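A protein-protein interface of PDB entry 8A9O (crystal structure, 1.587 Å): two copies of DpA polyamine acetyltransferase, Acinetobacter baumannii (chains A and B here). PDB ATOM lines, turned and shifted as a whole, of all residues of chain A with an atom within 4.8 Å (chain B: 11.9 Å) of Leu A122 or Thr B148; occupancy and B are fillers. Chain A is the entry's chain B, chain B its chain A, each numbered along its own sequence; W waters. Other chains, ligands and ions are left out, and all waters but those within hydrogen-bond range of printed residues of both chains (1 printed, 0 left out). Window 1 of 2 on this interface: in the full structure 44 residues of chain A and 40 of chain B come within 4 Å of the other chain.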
ATOM      1  N   LEU A  86       6.130 -28.711  26.054  1.00  0.00           N
ATOM      2  CA  LEU A  86       5.416 -29.965  26.274  1.00  0.00           C
ATOM      3  C   LEU A  86       6.359 -31.035  25.717  1.00  0.00           C
ATOM      4  O   LEU A  86       6.522 -31.165  24.486  1.00  0.00           O
ATOM      5  CB  LEU A  86       4.080 -29.932  25.534  1.00  0.00           C
ATOM      6  CG  LEU A  86       3.175 -31.123  25.745  1.00  0.00           C
ATOM      7  CD1 LEU A  86       1.768 -30.803  25.341  1.00  0.00           C
ATOM      8  CD2 LEU A  86       3.589 -32.266  24.884  1.00  0.00           C
ATOM      9  N   ILE A 120       2.858 -22.534  24.997  1.00  0.00           N
ATOM     10  CA  ILE A 120       3.319 -23.900  25.174  1.00  0.00           C
ATOM     11  C   ILE A 120       3.884 -24.279  23.801  1.00  0.00           C
ATOM     12  O   ILE A 120       3.204 -24.077  22.795  1.00  0.00           O
ATOM     13  CB  ILE A 120       2.233 -24.903  25.589  1.00  0.00           C
ATOM     14  CG1 ILE A 120       1.676 -24.539  26.982  1.00  0.00           C
ATOM     15  CG2 ILE A 120       2.844 -26.324  25.602  1.00  0.00           C
ATOM     16  CD1 ILE A 120       0.496 -25.400  27.413  1.00  0.00           C
ATOM     17  N   SER A 121       5.121 -24.747  23.741  1.00  0.00           N
ATOM     18  CA  SER A 121       5.737 -25.150  22.481  1.00  0.00           C
ATOM     19  C   SER A 121       6.108 -26.635  22.553  1.00  0.00           C
ATOM     20  O   SER A 121       6.358 -27.172  23.628  1.00  0.00           O
ATOM     21  CB  SER A 121       6.998 -24.328  22.214  1.00  0.00           C
ATOM     22  OG  SER A 121       6.614 -22.962  22.190  1.00  0.00           O
ATOM     23  N   LEU A 122       6.195 -27.274  21.393  1.00  0.00           N
ATOM     24  CA  LEU A 122       6.608 -28.667  21.345  1.00  0.00           C
ATOM     25  C   LEU A 122       7.162 -29.005  19.956  1.00  0.00           C
ATOM     26  O   LEU A 122       6.959 -28.247  19.006  1.00  0.00           O
ATOM     27  CB  LEU A 122       5.405 -29.584  21.673  1.00  0.00           C
ATOM     28  CG  LEU A 122       4.198 -29.520  20.733  1.00  0.00           C
ATOM     29  CD1 LEU A 122       4.372 -30.433  19.482  1.00  0.00           C
ATOM     30  CD2 LEU A 122       2.958 -29.953  21.442  1.00  0.00           C
ATOM     31  N   GLU A 123       7.808 -30.158  19.852  1.00  0.00           N
ATOM     32  CA  GLU A 123       8.276 -30.723  18.584  1.00  0.00           C
ATOM     33  C   GLU A 123       7.773 -32.153  18.525  1.00  0.00           C
ATOM     34  O   GLU A 123       7.925 -32.904  19.500  1.00  0.00           O
ATOM     35  CB  GLU A 123       9.819 -30.726  18.516  1.00  0.00           C
ATOM     36  N   THR A 124       7.203 -32.564  17.392  1.00  0.00           N
ATOM     37  CA  THR A 124       6.724 -33.937  17.235  1.00  0.00           C
ATOM     38  C   THR A 124       7.198 -34.442  15.876  1.00  0.00           C
ATOM     39  O   THR A 124       7.460 -33.625  14.992  1.00  0.00           O
ATOM     40  CB  THR A 124       5.185 -34.005  17.406  1.00  0.00           C
ATOM     41  OG1 THR A 124       4.758 -35.358  17.444  1.00  0.00           O
ATOM     42  CG2 THR A 124       4.427 -33.261  16.330  1.00  0.00           C
ATOM     43  N   TYR A 135      -2.792 -32.107  18.538  1.00  0.00           N
ATOM     44  CA  TYR A 135      -2.337 -30.747  18.811  1.00  0.00           C
ATOM     45  C   TYR A 135      -3.183 -29.709  18.107  1.00  0.00           C
ATOM     46  O   TYR A 135      -3.577 -28.718  18.729  1.00  0.00           O
ATOM     47  CB  TYR A 135      -0.841 -30.601  18.512  1.00  0.00           C
ATOM     48  CG  TYR A 135       0.002 -31.558  19.321  1.00  0.00           C
ATOM     49  CD1 TYR A 135      -0.265 -31.785  20.665  1.00  0.00           C
ATOM     50  CD2 TYR A 135       1.105 -32.186  18.761  1.00  0.00           C
ATOM     51  CE1 TYR A 135       0.509 -32.657  21.419  1.00  0.00           C
ATOM     52  CE2 TYR A 135       1.888 -33.064  19.505  1.00  0.00           C
ATOM     53  CZ  TYR A 135       1.586 -33.291  20.835  1.00  0.00           C
ATOM     54  OH  TYR A 135       2.374 -34.148  21.568  1.00  0.00           O
ATOM     55  N   PHE A 140      -3.083 -25.774  18.953  1.00  0.00           N
ATOM     56  CA  PHE A 140      -1.687 -25.568  18.577  1.00  0.00           C
ATOM     57  C   PHE A 140      -1.609 -25.270  17.084  1.00  0.00           C
ATOM     58  O   PHE A 140      -2.425 -25.767  16.300  1.00  0.00           O
ATOM     59  CB  PHE A 140      -0.822 -26.786  18.896  1.00  0.00           C
ATOM     60  CG  PHE A 140      -0.519 -26.979  20.365  1.00  0.00           C
ATOM     61  CD1 PHE A 140      -1.507 -27.395  21.244  1.00  0.00           C
ATOM     62  CD2 PHE A 140       0.767 -26.796  20.853  1.00  0.00           C
ATOM     63  CE1 PHE A 140      -1.223 -27.594  22.586  1.00  0.00           C
ATOM     64  CE2 PHE A 140       1.049 -26.996  22.194  1.00  0.00           C
ATOM     65  CZ  PHE A 140       0.052 -27.382  23.055  1.00  0.00           C
ATOM     66  N   ILE A 141      -0.617 -24.457  16.693  1.00  0.00           N
ATOM     67  CA  ILE A 141      -0.409 -24.067  15.312  1.00  0.00           C
ATOM     68  C   ILE A 141       0.932 -24.559  14.868  1.00  0.00           C
ATOM     69  O   ILE A 141       1.924 -24.429  15.585  1.00  0.00           O
ATOM     70  CB  ILE A 141      -0.534 -22.544  15.167  1.00  0.00           C
ATOM     71  CG1 ILE A 141      -1.904 -22.083  15.638  1.00  0.00           C
ATOM     72  CG2 ILE A 141      -0.291 -22.077  13.737  1.00  0.00           C
ATOM     73  CD1 ILE A 141      -1.796 -20.939  16.356  1.00  0.00           C
ATOM     74  N   ARG A 142       0.969 -25.155  13.698  1.00  0.00           N
ATOM     75  CA  ARG A 142       2.178 -25.648  13.053  1.00  0.00           C
ATOM     76  C   ARG A 142       3.075 -24.426  12.769  1.00  0.00           C
ATOM     77  O   ARG A 142       2.573 -23.402  12.286  1.00  0.00           O
ATOM     78  CB  ARG A 142       1.738 -26.226  11.701  1.00  0.00           C
ATOM     79  CG  ARG A 142       2.755 -27.067  11.013  1.00  0.00           C
ATOM     80  CD  ARG A 142       2.239 -27.408   9.638  1.00  0.00           C
ATOM     81  NE  ARG A 142       3.299 -27.952   8.801  1.00  0.00           N
ATOM     82  CZ  ARG A 142       3.402 -29.230   8.452  1.00  0.00           C
ATOM     83  NH1 ARG A 142       2.493 -30.112   8.855  1.00  0.00           N
ATOM     84  NH2 ARG A 142       4.409 -29.635   7.691  1.00  0.00           N
ATOM     85  N   ASP A 143       4.374 -24.512  13.082  1.00  0.00           N
ATOM     86  CA  ASP A 143       5.269 -23.380  12.859  1.00  0.00           C
ATOM     87  C   ASP A 143       6.571 -23.861  12.285  1.00  0.00           C
ATOM     88  O   ASP A 143       7.202 -24.725  12.878  1.00  0.00           O
ATOM     89  CB  ASP A 143       5.485 -22.643  14.197  1.00  0.00           C
ATOM     90  CG  ASP A 143       6.144 -21.275  14.092  1.00  0.00           C
ATOM     91  OD1 ASP A 143       7.045 -21.113  13.244  1.00  0.00           O
ATOM     92  OD2 ASP A 143       5.779 -20.376  14.888  1.00  0.00           O
ATOM     93  N   TYR B  83      21.123 -33.729  27.861  1.00  0.00           N
ATOM     94  CA  TYR B  83      21.761 -33.100  26.717  1.00  0.00           C
ATOM     95  C   TYR B  83      21.772 -31.587  26.967  1.00  0.00           C
ATOM     96  O   TYR B  83      21.274 -31.127  28.002  1.00  0.00           O
ATOM     97  CB  TYR B  83      21.057 -33.492  25.404  1.00  0.00           C
ATOM     98  CG  TYR B  83      19.638 -32.993  25.259  1.00  0.00           C
ATOM     99  CD1 TYR B  83      18.576 -33.699  25.807  1.00  0.00           C
ATOM    100  CD2 TYR B  83      19.349 -31.860  24.514  1.00  0.00           C
ATOM    101  CE1 TYR B  83      17.262 -33.266  25.644  1.00  0.00           C
ATOM    102  CE2 TYR B  83      18.043 -31.422  24.341  1.00  0.00           C
ATOM    103  CZ  TYR B  83      16.999 -32.139  24.896  1.00  0.00           C
ATOM    104  OH  TYR B  83      15.693 -31.730  24.737  1.00  0.00           O
ATOM    105  N   ILE B  85      20.972 -27.647  25.365  1.00  0.00           N
ATOM    106  CA  ILE B  85      20.350 -26.860  24.329  1.00  0.00           C
ATOM    107  C   ILE B  85      21.193 -25.591  24.202  1.00  0.00           C
ATOM    108  O   ILE B  85      21.415 -24.908  25.201  1.00  0.00           O
ATOM    109  CB  ILE B  85      18.896 -26.510  24.669  1.00  0.00           C
ATOM    110  CG1 ILE B  85      18.026 -27.765  24.588  1.00  0.00           C
ATOM    111  CG2 ILE B  85      18.351 -25.490  23.658  1.00  0.00           C
ATOM    112  CD1 ILE B  85      17.497 -28.177  25.841  1.00  0.00           C
ATOM    113  N   ARG B 119      24.107 -34.891  23.256  1.00  0.00           N
ATOM    114  CA  ARG B 119      24.250 -34.016  22.110  1.00  0.00           C
ATOM    115  C   ARG B 119      24.071 -32.565  22.558  1.00  0.00           C
ATOM    116  O   ARG B 119      23.728 -32.293  23.704  1.00  0.00           O
ATOM    117  CB  ARG B 119      23.094 -34.339  21.118  1.00  0.00           C
ATOM    118  CG  ARG B 119      21.689 -34.155  21.723  1.00  0.00           C
ATOM    119  CD  ARG B 119      20.605 -34.464  20.692  1.00  0.00           C
ATOM    120  NE  ARG B 119      19.275 -34.095  21.172  1.00  0.00           N
ATOM    121  CZ  ARG B 119      18.455 -34.916  21.816  1.00  0.00           C
ATOM    122  NH1 ARG B 119      18.817 -36.170  22.060  1.00  0.00           N
ATOM    123  NH2 ARG B 119      17.272 -34.488  22.234  1.00  0.00           N
ATOM    124  N   SER B 121      21.663 -29.540  21.057  1.00  0.00           N
ATOM    125  CA  SER B 121      20.606 -29.270  20.081  1.00  0.00           C
ATOM    126  C   SER B 121      20.292 -27.784  20.081  1.00  0.00           C
ATOM    127  O   SER B 121      20.469 -27.111  21.098  1.00  0.00           O
ATOM    128  CB  SER B 121      19.351 -30.067  20.422  1.00  0.00           C
ATOM    129  OG  SER B 121      19.696 -31.446  20.395  1.00  0.00           O
ATOM    130  N   LEU B 122      19.782 -27.278  18.964  1.00  0.00           N
ATOM    131  CA  LEU B 122      19.387 -25.881  18.889  1.00  0.00           C
ATOM    132  C   LEU B 122      18.317 -25.673  17.851  1.00  0.00           C
ATOM    133  O   LEU B 122      18.093 -26.547  17.034  1.00  0.00           O
ATOM    134  CB  LEU B 122      20.633 -24.998  18.585  1.00  0.00           C
ATOM    135  CG  LEU B 122      21.337 -25.246  17.247  1.00  0.00           C
ATOM    136  CD1 LEU B 122      20.658 -24.496  16.082  1.00  0.00           C
ATOM    137  CD2 LEU B 122      22.742 -24.785  17.305  1.00  0.00           C
ATOM    138  N   GLU B 123      17.693 -24.507  17.868  1.00  0.00           N
ATOM    139  CA  GLU B 123      16.754 -24.064  16.852  1.00  0.00           C
ATOM    140  C   GLU B 123      17.223 -22.679  16.382  1.00  0.00           C
ATOM    141  O   GLU B 123      17.538 -21.812  17.192  1.00  0.00           O
ATOM    142  CB  GLU B 123      15.305 -23.972  17.389  1.00  0.00           C
ATOM    143  N   THR B 124      17.266 -22.477  15.064  1.00  0.00           N
ATOM    144  CA  THR B 124      17.633 -21.189  14.497  1.00  0.00           C
ATOM    145  C   THR B 124      16.615 -20.854  13.418  1.00  0.00           C
ATOM    146  O   THR B 124      15.975 -21.763  12.899  1.00  0.00           O
ATOM    147  CB  THR B 124      19.069 -21.234  13.964  1.00  0.00           C
ATOM    148  OG1 THR B 124      19.474 -19.915  13.588  1.00  0.00           O
ATOM    149  CG2 THR B 124      19.260 -22.195  12.778  1.00  0.00           C
ATOM    150  N   GLN B 125      16.456 -19.572  13.051  1.00  0.00           N
ATOM    151  CA  GLN B 125      15.472 -19.212  12.011  1.00  0.00           C
ATOM    152  C   GLN B 125      15.812 -19.931  10.685  1.00  0.00           C
ATOM    153  O   GLN B 125      16.985 -20.032  10.337  1.00  0.00           O
ATOM    154  CB  GLN B 125      15.436 -17.700  11.811  1.00  0.00           C
ATOM    155  CG  GLN B 125      14.833 -16.958  12.986  1.00  0.00           C
ATOM    156  CD  GLN B 125      15.030 -15.470  12.881  1.00  0.00           C
ATOM    157  OE1 GLN B 125      16.155 -14.938  12.932  1.00  0.00           O
ATOM    158  NE2 GLN B 125      13.945 -14.768  12.709  1.00  0.00           N
ATOM    159  N   SER B 126      14.804 -20.473   9.990  1.00  0.00           N
ATOM    160  CA  SER B 126      15.026 -21.158   8.726  1.00  0.00           C
ATOM    161  C   SER B 126      15.641 -20.238   7.675  1.00  0.00           C
ATOM    162  O   SER B 126      16.321 -20.725   6.784  1.00  0.00           O
ATOM    163  CB  SER B 126      13.722 -21.775   8.215  1.00  0.00           C
ATOM    164  OG  SER B 126      13.115 -22.572   9.222  1.00  0.00           O
ATOM    165  N   ARG B 142      21.258 -30.762  10.280  1.00  0.00           N
ATOM    166  CA  ARG B 142      19.896 -30.260  10.207  1.00  0.00           C
ATOM    167  C   ARG B 142      18.916 -31.412  10.524  1.00  0.00           C
ATOM    168  O   ARG B 142      19.056 -32.503   9.980  1.00  0.00           O
ATOM    169  CB  ARG B 142      19.645 -29.713   8.785  1.00  0.00           C
ATOM    170  CG  ARG B 142      18.744 -28.495   8.715  1.00  0.00           C
ATOM    171  CD  ARG B 142      18.645 -27.894   7.310  1.00  0.00           C
ATOM    172  NE  ARG B 142      19.950 -27.428   6.845  1.00  0.00           N
ATOM    173  CZ  ARG B 142      20.199 -26.210   6.373  1.00  0.00           C
ATOM    174  NH1 ARG B 142      19.224 -25.317   6.270  1.00  0.00           N
ATOM    175  NH2 ARG B 142      21.426 -25.881   5.991  1.00  0.00           N
ATOM    176  N   GLU B 145      13.215 -34.490  10.636  1.00  0.00           N
ATOM    177  CA  GLU B 145      12.192 -35.420  11.107  1.00  0.00           C
ATOM    178  C   GLU B 145      11.128 -34.803  11.982  1.00  0.00           C
ATOM    179  O   GLU B 145      10.100 -35.447  12.179  1.00  0.00           O
ATOM    180  CB  GLU B 145      12.849 -36.537  11.938  1.00  0.00           C
ATOM    181  CG  GLU B 145      14.046 -37.212  11.300  1.00  0.00           C
ATOM    182  CD  GLU B 145      13.716 -38.459  10.511  1.00  0.00           C
ATOM    183  OE1 GLU B 145      14.393 -39.490  10.725  1.00  0.00           O
ATOM    184  OE2 GLU B 145      12.778 -38.408   9.680  1.00  0.00           O
ATOM    185  N   PHE B 146      11.377 -33.629  12.592  1.00  0.00           N
ATOM    186  CA  PHE B 146      10.415 -33.056  13.546  1.00  0.00           C
ATOM    187  C   PHE B 146       9.764 -31.760  13.082  1.00  0.00           C
ATOM    188  O   PHE B 146      10.353 -30.996  12.311  1.00  0.00           O
ATOM    189  CB  PHE B 146      11.066 -32.849  14.943  1.00  0.00           C
ATOM    190  CG  PHE B 146      11.328 -34.119  15.718  1.00  0.00           C
ATOM    191  CD1 PHE B 146      12.415 -34.916  15.422  1.00  0.00           C
ATOM    192  CD2 PHE B 146      10.484 -34.515  16.741  1.00  0.00           C
ATOM    193  CE1 PHE B 146      12.636 -36.095  16.113  1.00  0.00           C
ATOM    194  CE2 PHE B 146      10.699 -35.707  17.420  1.00  0.00           C
ATOM    195  CZ  PHE B 146      11.787 -36.479  17.116  1.00  0.00           C
ATOM    196  N   GLN B 147       8.556 -31.506  13.579  1.00  0.00           N
ATOM    197  CA  GLN B 147       7.749 -30.333  13.288  1.00  0.00           C
ATOM    198  C   GLN B 147       7.414 -29.598  14.595  1.00  0.00           C
ATOM    199  O   GLN B 147       6.930 -30.227  15.534  1.00  0.00           O
ATOM    200  CB  GLN B 147       6.445 -30.766  12.614  1.00  0.00           C
ATOM    201  CG  GLN B 147       5.483 -29.618  12.344  1.00  0.00           C
ATOM    202  CD  GLN B 147       6.061 -28.577  11.408  1.00  0.00           C
ATOM    203  OE1 GLN B 147       6.135 -27.381  11.737  1.00  0.00           O
ATOM    204  NE2 GLN B 147       6.508 -29.011  10.245  1.00  0.00           N
ATOM    205  N   THR B 148       7.621 -28.283  14.634  1.00  0.00           N
ATOM    206  CA  THR B 148       7.296 -27.486  15.806  1.00  0.00           C
ATOM    207  C   THR B 148       5.850 -27.040  15.787  1.00  0.00           C
ATOM    208  O   THR B 148       5.330 -26.675  14.725  1.00  0.00           O
ATOM    209  CB  THR B 148       8.177 -26.235  15.859  1.00  0.00           C
ATOM    210  OG1 THR B 148       9.540 -26.611  15.891  1.00  0.00           O
ATOM    211  CG2 THR B 148       7.862 -25.339  17.059  1.00  0.00           C
ATOM    212  N   PHE B 149       5.195 -27.047  16.961  1.00  0.00           N
ATOM    213  CA  PHE B 149       3.845 -26.510  17.124  1.00  0.00           C
ATOM    214  C   PHE B 149       3.838 -25.583  18.341  1.00  0.00           C
ATOM    215  O   PHE B 149       4.552 -25.859  19.315  1.00  0.00           O
ATOM    216  CB  PHE B 149       2.829 -27.642  17.423  1.00  0.00           C
ATOM    217  CG  PHE B 149       2.404 -28.476  16.237  1.00  0.00           C
ATOM    218  CD1 PHE B 149       3.202 -29.503  15.771  1.00  0.00           C
ATOM    219  CD2 PHE B 149       1.193 -28.256  15.624  1.00  0.00           C
ATOM    220  CE1 PHE B 149       2.802 -30.269  14.676  1.00  0.00           C
ATOM    221  CE2 PHE B 149       0.798 -29.018  14.523  1.00  0.00           C
ATOM    222  CZ  PHE B 149       1.598 -30.015  14.061  1.00  0.00           C
ATOM    223  N   HIS B 150       3.049 -24.519  18.302  1.00  0.00           N
ATOM    224  CA  HIS B 150       2.924 -23.600  19.436  1.00  0.00           C
ATOM    225  C   HIS B 150       1.462 -23.366  19.777  1.00  0.00           C
ATOM    226  O   HIS B 150       0.624 -23.237  18.880  1.00  0.00           O
ATOM    227  CB  HIS B 150       3.516 -22.215  19.093  1.00  0.00           C
ATOM    228  CG  HIS B 150       4.943 -22.230  18.701  1.00  0.00           C
ATOM    229  ND1 HIS B 150       5.942 -22.518  19.607  1.00  0.00           N
ATOM    230  CD2 HIS B 150       5.504 -21.927  17.512  1.00  0.00           C
ATOM    231  CE1 HIS B 150       7.077 -22.434  18.932  1.00  0.00           C
ATOM    232  NE2 HIS B 150       6.862 -22.096  17.661  1.00  0.00           N
ATOM    233  N   CYS B 151       1.161 -23.266  21.071  1.00  0.00           N
ATOM    234  CA  CYS B 151      -0.143 -22.868  21.555  1.00  0.00           C
ATOM    235  C   CYS B 151       0.091 -21.542  22.241  1.00  0.00           C
ATOM    236  O   CYS B 151       0.746 -21.483  23.279  1.00  0.00           O
ATOM    237  CB  CYS B 151      -0.752 -23.884  22.506  1.00  0.00           C
ATOM    238  SG  CYS B 151      -2.295 -23.314  23.254  1.00  0.00           S
ATOM    239  N   PHE B 152      -0.445 -20.459  21.679  1.00  0.00           N
ATOM    240  CA  PHE B 152      -0.143 -19.106  22.220  1.00  0.00           C
ATOM    241  C   PHE B 152      -1.023 -18.749  23.432  1.00  0.00           C
ATOM    242  O   PHE B 152      -0.932 -17.636  23.913  1.00  0.00           O
ATOM    243  CB  PHE B 152      -0.134 -18.091  21.068  1.00  0.00           C
ATOM    244  CG  PHE B 152       0.954 -18.351  20.061  1.00  0.00           C
ATOM    245  CD1 PHE B 152       2.275 -18.053  20.354  1.00  0.00           C
ATOM    246  CD2 PHE B 152       0.667 -18.927  18.835  1.00  0.00           C
ATOM    247  CE1 PHE B 152       3.280 -18.305  19.436  1.00  0.00           C
ATOM    248  CE2 PHE B 152       1.673 -19.179  17.919  1.00  0.00           C
ATOM    249  CZ  PHE B 152       2.977 -18.865  18.217  1.00  0.00           C
ATOM    250  N   LEU B 153      -1.788 -19.702  23.960  1.00  0.00           N
ATOM    251  CA  LEU B 153      -2.538 -19.448  25.222  1.00  0.00           C
ATOM    252  C   LEU B 153      -3.342 -18.143  25.112  1.00  0.00           C
ATOM    253  O   LEU B 153      -3.799 -17.659  26.161  1.00  0.00           O
ATOM    254  CB  LEU B 153      -1.523 -19.377  26.369  1.00  0.00           C
ATOM    255  CG  LEU B 153      -0.647 -20.611  26.571  1.00  0.00           C
ATOM    256  CD1 LEU B 153       0.314 -20.396  27.726  1.00  0.00           C
ATOM    257  CD2 LEU B 153      -1.496 -21.848  26.806  1.00  0.00           C
HETATM  258  O   HOH W   1       9.305 -26.906  12.553  1.00  0.00           O
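NE2 of His B150 lies close to OD2 of Asp A143, 3.4 Å away. NE2 of Gln B147 sits close to NH2 of Arg A142 (3.4 Å). The side-chain hydroxyl of Ser A121 sits at hydrogen-bond distance from a ring nitrogen (ND1) of His B150 (2.7 Å). The backbone NH (N) of Asp A143 is in hydrogen-bond range of the backbone carbonyl oxygen (O) of Thr B148 (2.9 Å). The side-chain amide oxygen (OE1) of Gln B147 sits close to the backbone carbonyl oxygen (O) of Asp A143 (3.1 Å). O of Thr A124 lies within hydrogen-bond range of N of Gln B147 (2.8 Å). The backbone NH (N) of Phe B149 sits at hydrogen-bond distance from the backbone carbonyl oxygen (O) of Leu A122 (3.0 Å). N of Cys B151 sits at hydrogen-bond distance from O of Ile A120, 2.8 Å away. The backbone NH (N) of Ile A141 sits at hydrogen-bond distance from the backbone carbonyl oxygen (O) of His B150 (2.8 Å).
Hydrophobic or aromatic side chains of chain A that line the printed part of chain B: Leu A122, Phe A140 and Ile A141. Hydrophobic or aromatic side chains of chain B that line the printed part of chain A: Phe B146, Phe B149 and His B150. Among the printed residues, 21 pairs touch across the chains.
Positions printed for both chains: 121, 122, 123, 124 and 142.
O of Ser A121 sits at hydrogen-bond distance from N of Leu A86, 2.9 Å away. The backbone NH (N) of Phe A140 lies within hydrogen-bond range of the backbone carbonyl oxygen (O) of Tyr A135. SG of Cys B151 sits close to N of Leu B153.
Phe B149 touches Ser A121. O of Gln B147 touches O of Leu A122, 3.997 Å away. CA of Thr B148 touches O of Leu A122 (3.3 Å). Phe B146 touches Thr A124 (CA to O, 3.3 Å). CG2 of Thr A124 touches CE1 of Phe B149, at 3.8 Å. His B150 touches Phe A140. N of Cys B151 touches CD2 of Phe A140 (3.6 Å). Phe B149 touches Ile A141 (CA to O, 3.2 Å). Arg A142 touches Thr B148 (CA to O, 3.7 Å). Arg A142 touches Phe B149 (N to CD2, 3.7 Å).
Water W1 lies within hydrogen-bond range of N of Thr B148 (3.0 Å), O of Asp A143 (3.0 Å) and OE1 of Gln B147 (3.3 Å).
Of the printed residues of chain B, Leu A122 touches Gln B147 (3.997 Å), Thr B148 (3.3 Å) and Phe B149 (3.0 Å). Of chain A, only Leu A122, Arg A142 and Asp A143 come within 4 Å of Thr B148. No residue of chain B comes within 4 Å of Leu A86. Of the printed residues of chain B, Thr A124 touches Phe B146, Gln B147 and Phe B149. Tyr A135 touches none of the printed residues of chain B. Arg A142 touches just these residues of chain B: Gln B147, Thr B148 and Phe B149. Of the printed residues of chain B, Phe A140 touches His B150 (3.3 Å) and Cys B151 (3.6 Å). Of the printed residues of chain A, Phe B149 touches Ser A121, Leu A122, Thr A124, Ile A141 and Arg A142. The nearest printed residue of chain A that does not touch Cys B151 is Ile A141 (4.9 Å).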
